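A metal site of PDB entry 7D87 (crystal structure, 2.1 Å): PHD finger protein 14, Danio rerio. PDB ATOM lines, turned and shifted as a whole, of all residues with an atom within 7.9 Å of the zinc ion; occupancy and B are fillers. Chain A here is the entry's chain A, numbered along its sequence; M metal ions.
The backbone carbonyl oxygen of Thr 142 is in hydrogen-bond range of a ring nitrogen (NE2) of His 158 (2.7 Å).
SG of Cys 131 sits close to N of Leu 133 (3.4 Å).
The backbone NH (N) of Cys 131 is in hydrogen-bond range of the backbone carbonyl oxygen (O) of Ala 140.
The backbone NH (N) of Cys 131 sits close to the side-chain sulfur (SG) of Cys 145 (3.6 Å).
Four residues have an atom within 4 Å of the zinc ion: Cys 131, Cys 134, His 158 and Cys 161.
The zinc ion is bound by ND1 of His 158 (2.1 Å), SG of Cys 131 (2.3 Å), SG of Cys 134 (2.3 Å) and SG of Cys 161 (2.3 Å).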
ATOM      1  N   LEU A  77      -5.074  30.132   8.385  1.00  0.00           N
ATOM      2  CA  LEU A  77      -4.731  29.015   9.262  1.00  0.00           C
ATOM      3  C   LEU A  77      -3.312  28.470   9.067  1.00  0.00           C
ATOM      4  O   LEU A  77      -2.950  27.507   9.761  1.00  0.00           O
ATOM      5  CB  LEU A  77      -5.759  27.881   9.077  1.00  0.00           C
ATOM      6  CG  LEU A  77      -7.221  28.193   9.407  1.00  0.00           C
ATOM      7  CD1 LEU A  77      -8.125  27.047   8.972  1.00  0.00           C
ATOM      8  CD2 LEU A  77      -7.382  28.438  10.880  1.00  0.00           C
ATOM      9  N   CYS A  78      -2.516  29.028   8.169  1.00  0.00           N
ATOM     10  CA  CYS A  78      -1.175  28.503   7.918  1.00  0.00           C
ATOM     11  C   CYS A  78      -0.408  29.529   7.107  1.00  0.00           C
ATOM     12  O   CYS A  78      -1.022  30.456   6.565  1.00  0.00           O
ATOM     13  CB  CYS A  78      -1.232  27.148   7.177  1.00  0.00           C
ATOM     14  SG  CYS A  78      -1.503  27.284   5.390  1.00  0.00           S
ATOM     15  N   PRO A  79       0.912  29.384   7.011  1.00  0.00           N
ATOM     16  CA  PRO A  79       1.744  30.352   6.271  1.00  0.00           C
ATOM     17  C   PRO A  79       1.954  30.049   4.803  1.00  0.00           C
ATOM     18  O   PRO A  79       2.588  30.857   4.113  1.00  0.00           O
ATOM     19  CB  PRO A  79       3.086  30.281   7.005  1.00  0.00           C
ATOM     20  CG  PRO A  79       3.184  28.855   7.431  1.00  0.00           C
ATOM     21  CD  PRO A  79       1.750  28.465   7.808  1.00  0.00           C
ATOM     22  N   SER A  80       1.438  28.939   4.293  1.00  0.00           N
ATOM     23  CA  SER A  80       1.692  28.567   2.903  1.00  0.00           C
ATOM     24  C   SER A  80       0.863  29.421   1.943  1.00  0.00           C
ATOM     25  O   SER A  80      -0.280  29.782   2.236  1.00  0.00           O
ATOM     26  CB  SER A  80       1.367  27.088   2.692  1.00  0.00           C
ATOM     27  OG  SER A  80       1.487  26.746   1.328  1.00  0.00           O
ATOM     28  N   GLU A 130       3.505  25.539  18.338  1.00  0.00           N
ATOM     29  CA  GLU A 130       4.586  25.721  17.383  1.00  0.00           C
ATOM     30  C   GLU A 130       4.548  24.597  16.363  1.00  0.00           C
ATOM     31  O   GLU A 130       4.471  23.414  16.729  1.00  0.00           O
ATOM     32  CB  GLU A 130       5.943  25.756  18.088  1.00  0.00           C
ATOM     33  CG  GLU A 130       7.122  25.847  17.123  1.00  0.00           C
ATOM     34  CD  GLU A 130       8.465  25.920  17.846  1.00  0.00           C
ATOM     35  OE1 GLU A 130       8.469  26.261  19.042  1.00  0.00           O
ATOM     36  OE2 GLU A 130       9.497  25.637  17.205  1.00  0.00           O
ATOM     37  N   CYS A 131       4.593  24.951  15.082  1.00  0.00           N
ATOM     38  CA  CYS A 131       4.584  23.929  14.044  1.00  0.00           C
ATOM     39  C   CYS A 131       5.948  23.266  14.004  1.00  0.00           C
ATOM     40  O   CYS A 131       6.956  23.949  13.802  1.00  0.00           O
ATOM     41  CB  CYS A 131       4.241  24.537  12.687  1.00  0.00           C
ATOM     42  SG  CYS A 131       4.592  23.416  11.277  1.00  0.00           S
ATOM     43  N   SER A 132       5.993  21.953  14.208  1.00  0.00           N
ATOM     44  CA  SER A 132       7.266  21.250  14.239  1.00  0.00           C
ATOM     45  C   SER A 132       7.832  20.948  12.855  1.00  0.00           C
ATOM     46  O   SER A 132       8.957  20.453  12.765  1.00  0.00           O
ATOM     47  CB  SER A 132       7.117  19.927  15.026  1.00  0.00           C
ATOM     48  OG  SER A 132       6.156  19.080  14.422  1.00  0.00           O
ATOM     49  N   LEU A 133       7.102  21.239  11.775  1.00  0.00           N
ATOM     50  CA  LEU A 133       7.591  20.939  10.438  1.00  0.00           C
ATOM     51  C   LEU A 133       7.865  22.175   9.598  1.00  0.00           C
ATOM     52  O   LEU A 133       8.295  22.016   8.448  1.00  0.00           O
ATOM     53  CB  LEU A 133       6.605  20.047   9.682  1.00  0.00           C
ATOM     54  CG  LEU A 133       6.284  18.734  10.354  1.00  0.00           C
ATOM     55  CD1 LEU A 133       5.146  18.027   9.641  1.00  0.00           C
ATOM     56  CD2 LEU A 133       7.534  17.897  10.389  1.00  0.00           C
ATOM     57  N   CYS A 134       7.584  23.394  10.093  1.00  0.00           N
ATOM     58  CA  CYS A 134       7.915  24.583   9.319  1.00  0.00           C
ATOM     59  C   CYS A 134       9.394  24.578   8.966  1.00  0.00           C
ATOM     60  O   CYS A 134      10.257  24.406   9.835  1.00  0.00           O
ATOM     61  CB  CYS A 134       7.569  25.855  10.103  1.00  0.00           C
ATOM     62  SG  CYS A 134       5.972  26.604   9.701  1.00  0.00           S
ATOM     63  N   GLU A 135       9.692  24.784   7.691  1.00  0.00           N
ATOM     64  CA  GLU A 135      11.080  24.982   7.291  1.00  0.00           C
ATOM     65  C   GLU A 135      11.561  26.396   7.602  1.00  0.00           C
ATOM     66  O   GLU A 135      12.743  26.610   7.863  1.00  0.00           O
ATOM     67  CB  GLU A 135      11.248  24.654   5.812  1.00  0.00           C
ATOM     68  CG  GLU A 135      10.174  23.706   5.262  1.00  0.00           C
ATOM     69  CD  GLU A 135      10.703  22.712   4.241  1.00  0.00           C
ATOM     70  OE1 GLU A 135      11.371  21.741   4.640  1.00  0.00           O
ATOM     71  OE2 GLU A 135      10.457  22.923   3.029  1.00  0.00           O
ATOM     72  N   ASP A 136      10.660  27.380   7.586  1.00  0.00           N
ATOM     73  CA  ASP A 136      11.035  28.747   7.921  1.00  0.00           C
ATOM     74  C   ASP A 136      10.462  29.021   9.314  1.00  0.00           C
ATOM     75  O   ASP A 136       9.265  29.291   9.455  1.00  0.00           O
ATOM     76  CB  ASP A 136      10.511  29.735   6.876  1.00  0.00           C
ATOM     77  CG  ASP A 136      11.018  31.165   7.084  1.00  0.00           C
ATOM     78  OD1 ASP A 136      11.607  31.470   8.146  1.00  0.00           O
ATOM     79  OD2 ASP A 136      10.814  31.995   6.182  1.00  0.00           O
ATOM     80  N   PHE A 139       7.706  31.432  10.737  1.00  0.00           N
ATOM     81  CA  PHE A 139       6.280  31.232  10.607  1.00  0.00           C
ATOM     82  C   PHE A 139       5.780  30.087  11.459  1.00  0.00           C
ATOM     83  O   PHE A 139       4.595  29.783  11.409  1.00  0.00           O
ATOM     84  CB  PHE A 139       5.905  30.997   9.134  1.00  0.00           C
ATOM     85  CG  PHE A 139       6.290  32.133   8.235  1.00  0.00           C
ATOM     86  CD1 PHE A 139       5.458  33.231   8.074  1.00  0.00           C
ATOM     87  CD2 PHE A 139       7.494  32.112   7.560  1.00  0.00           C
ATOM     88  CE1 PHE A 139       5.816  34.287   7.249  1.00  0.00           C
ATOM     89  CE2 PHE A 139       7.873  33.179   6.728  1.00  0.00           C
ATOM     90  CZ  PHE A 139       7.034  34.262   6.581  1.00  0.00           C
ATOM     91  N   ALA A 140       6.657  29.448  12.242  1.00  0.00           N
ATOM     92  CA  ALA A 140       6.247  28.253  12.982  1.00  0.00           C
ATOM     93  C   ALA A 140       5.122  28.539  13.957  1.00  0.00           C
ATOM     94  O   ALA A 140       4.404  27.613  14.351  1.00  0.00           O
ATOM     95  CB  ALA A 140       7.449  27.644  13.720  1.00  0.00           C
ATOM     96  N   ARG A 141       4.917  29.801  14.338  1.00  0.00           N
ATOM     97  CA  ARG A 141       3.848  30.150  15.275  1.00  0.00           C
ATOM     98  C   ARG A 141       2.800  31.054  14.651  1.00  0.00           C
ATOM     99  O   ARG A 141       2.078  31.741  15.367  1.00  0.00           O
ATOM    100  CB  ARG A 141       4.444  30.784  16.534  1.00  0.00           C
ATOM    101  CG  ARG A 141       5.681  30.054  16.995  1.00  0.00           C
ATOM    102  CD  ARG A 141       5.742  29.883  18.481  1.00  0.00           C
ATOM    103  NE  ARG A 141       4.460  29.482  19.028  1.00  0.00           N
ATOM    104  CZ  ARG A 141       4.330  28.776  20.146  1.00  0.00           C
ATOM    105  NH1 ARG A 141       5.413  28.384  20.810  1.00  0.00           N
ATOM    106  NH2 ARG A 141       3.125  28.448  20.582  1.00  0.00           N
ATOM    107  N   THR A 142       2.706  31.079  13.329  1.00  0.00           N
ATOM    108  CA  THR A 142       1.541  31.669  12.681  1.00  0.00           C
ATOM    109  C   THR A 142       0.459  30.604  12.551  1.00  0.00           C
ATOM    110  O   THR A 142       0.690  29.412  12.754  1.00  0.00           O
ATOM    111  CB  THR A 142       1.912  32.258  11.317  1.00  0.00           C
ATOM    112  OG1 THR A 142       2.366  31.221  10.442  1.00  0.00           O
ATOM    113  CG2 THR A 142       3.008  33.289  11.453  1.00  0.00           C
ATOM    114  N   VAL A 144      -2.680  28.004  12.670  1.00  0.00           N
ATOM    115  CA  VAL A 144      -3.198  27.016  13.606  1.00  0.00           C
ATOM    116  C   VAL A 144      -2.590  25.666  13.245  1.00  0.00           C
ATOM    117  O   VAL A 144      -2.573  25.294  12.068  1.00  0.00           O
ATOM    118  CB  VAL A 144      -4.733  26.988  13.580  1.00  0.00           C
ATOM    119  CG1 VAL A 144      -5.331  25.879  14.461  1.00  0.00           C
ATOM    120  CG2 VAL A 144      -5.283  28.367  14.009  1.00  0.00           C
ATOM    121  N   CYS A 145      -2.070  24.957  14.243  1.00  0.00           N
ATOM    122  CA  CYS A 145      -1.551  23.599  14.089  1.00  0.00           C
ATOM    123  C   CYS A 145      -2.603  22.567  14.438  1.00  0.00           C
ATOM    124  O   CYS A 145      -3.469  22.788  15.291  1.00  0.00           O
ATOM    125  CB  CYS A 145      -0.349  23.364  15.012  1.00  0.00           C
ATOM    126  SG  CYS A 145       1.096  24.280  14.560  1.00  0.00           S
ATOM    127  N   PHE A 156       2.842  18.612  16.839  1.00  0.00           N
ATOM    128  CA  PHE A 156       2.000  19.631  16.211  1.00  0.00           C
ATOM    129  C   PHE A 156       2.590  20.113  14.883  1.00  0.00           C
ATOM    130  O   PHE A 156       3.812  20.207  14.713  1.00  0.00           O
ATOM    131  CB  PHE A 156       1.790  20.857  17.138  1.00  0.00           C
ATOM    132  CG  PHE A 156       1.338  20.500  18.544  1.00  0.00           C
ATOM    133  CD1 PHE A 156       0.097  19.920  18.753  1.00  0.00           C
ATOM    134  CD2 PHE A 156       2.152  20.756  19.635  1.00  0.00           C
ATOM    135  CE1 PHE A 156      -0.322  19.585  20.025  1.00  0.00           C
ATOM    136  CE2 PHE A 156       1.747  20.416  20.916  1.00  0.00           C
ATOM    137  CZ  PHE A 156       0.506  19.828  21.110  1.00  0.00           C
ATOM    138  N   PHE A 157       1.700  20.430  13.939  1.00  0.00           N
ATOM    139  CA  PHE A 157       2.128  20.963  12.659  1.00  0.00           C
ATOM    140  C   PHE A 157       0.963  21.629  11.948  1.00  0.00           C
ATOM    141  O   PHE A 157      -0.197  21.264  12.145  1.00  0.00           O
ATOM    142  CB  PHE A 157       2.694  19.861  11.752  1.00  0.00           C
ATOM    143  CG  PHE A 157       2.089  18.496  12.028  1.00  0.00           C
ATOM    144  CD1 PHE A 157       0.766  18.232  11.746  1.00  0.00           C
ATOM    145  CD2 PHE A 157       2.860  17.499  12.613  1.00  0.00           C
ATOM    146  CE1 PHE A 157       0.212  16.979  12.030  1.00  0.00           C
ATOM    147  CE2 PHE A 157       2.306  16.250  12.888  1.00  0.00           C
ATOM    148  CZ  PHE A 157       0.989  15.997  12.599  1.00  0.00           C
ATOM    149  N   HIS A 158       1.313  22.607  11.108  1.00  0.00           N
ATOM    150  CA  HIS A 158       0.375  23.186  10.154  1.00  0.00           C
ATOM    151  C   HIS A 158      -0.163  22.109   9.206  1.00  0.00           C
ATOM    152  O   HIS A 158       0.541  21.174   8.839  1.00  0.00           O
ATOM    153  CB  HIS A 158       1.087  24.264   9.334  1.00  0.00           C
ATOM    154  CG  HIS A 158       1.454  25.479  10.128  1.00  0.00           C
ATOM    155  ND1 HIS A 158       2.756  25.924  10.241  1.00  0.00           N
ATOM    156  CD2 HIS A 158       0.692  26.342  10.837  1.00  0.00           C
ATOM    157  CE1 HIS A 158       2.781  27.006  10.999  1.00  0.00           C
ATOM    158  NE2 HIS A 158       1.539  27.284  11.376  1.00  0.00           N
ATOM    159  N   VAL A 159      -1.435  22.256   8.794  1.00  0.00           N
ATOM    160  CA  VAL A 159      -2.013  21.239   7.920  1.00  0.00           C
ATOM    161  C   VAL A 159      -1.232  21.135   6.603  1.00  0.00           C
ATOM    162  O   VAL A 159      -0.991  20.045   6.103  1.00  0.00           O
ATOM    163  CB  VAL A 159      -3.507  21.525   7.653  1.00  0.00           C
ATOM    164  CG1 VAL A 159      -4.067  20.527   6.654  1.00  0.00           C
ATOM    165  CG2 VAL A 159      -4.319  21.463   8.958  1.00  0.00           C
ATOM    166  N   THR A 160      -0.819  22.279   6.039  1.00  0.00           N
ATOM    167  CA  THR A 160      -0.107  22.265   4.766  1.00  0.00           C
ATOM    168  C   THR A 160       1.341  21.821   4.905  1.00  0.00           C
ATOM    169  O   THR A 160       1.933  21.335   3.931  1.00  0.00           O
ATOM    170  CB  THR A 160      -0.145  23.649   4.142  1.00  0.00           C
ATOM    171  OG1 THR A 160       0.083  24.615   5.174  1.00  0.00           O
ATOM    172  CG2 THR A 160      -1.498  23.891   3.478  1.00  0.00           C
ATOM    173  N   CYS A 161       1.951  22.035   6.078  1.00  0.00           N
ATOM    174  CA  CYS A 161       3.279  21.467   6.304  1.00  0.00           C
ATOM    175  C   CYS A 161       3.193  19.946   6.423  1.00  0.00           C
ATOM    176  O   CYS A 161       4.031  19.225   5.878  1.00  0.00           O
ATOM    177  CB  CYS A 161       3.937  22.090   7.534  1.00  0.00           C
ATOM    178  SG  CYS A 161       4.316  23.887   7.429  1.00  0.00           S
ATOM    179  N   ALA A 162       2.153  19.445   7.108  1.00  0.00           N
ATOM    180  CA  ALA A 162       1.933  18.000   7.187  1.00  0.00           C
ATOM    181  C   ALA A 162       1.598  17.420   5.818  1.00  0.00           C
ATOM    182  O   ALA A 162       2.061  16.321   5.476  1.00  0.00           O
ATOM    183  CB  ALA A 162       0.817  17.702   8.210  1.00  0.00           C
ATOM    184  N   ARG A 164       2.767  18.351   2.982  1.00  0.00           N
ATOM    185  CA  ARG A 164       4.012  18.287   2.230  1.00  0.00           C
ATOM    186  C   ARG A 164       4.796  17.022   2.601  1.00  0.00           C
ATOM    187  O   ARG A 164       5.396  16.385   1.734  1.00  0.00           O
ATOM    188  CB  ARG A 164       4.823  19.546   2.509  1.00  0.00           C
ATOM    189  CG  ARG A 164       6.155  19.647   1.800  1.00  0.00           C
ATOM    190  CD  ARG A 164       6.977  20.815   2.356  1.00  0.00           C
ATOM    191  NE  ARG A 164       7.500  20.506   3.684  1.00  0.00           N
ATOM    192  CZ  ARG A 164       7.252  21.224   4.783  1.00  0.00           C
ATOM    193  NH1 ARG A 164       6.506  22.313   4.737  1.00  0.00           N
ATOM    194  NH2 ARG A 164       7.792  20.844   5.945  1.00  0.00           N
HETATM  195 ZN    ZN M   1       4.464  24.872   9.530  1.00  0.00          ZN
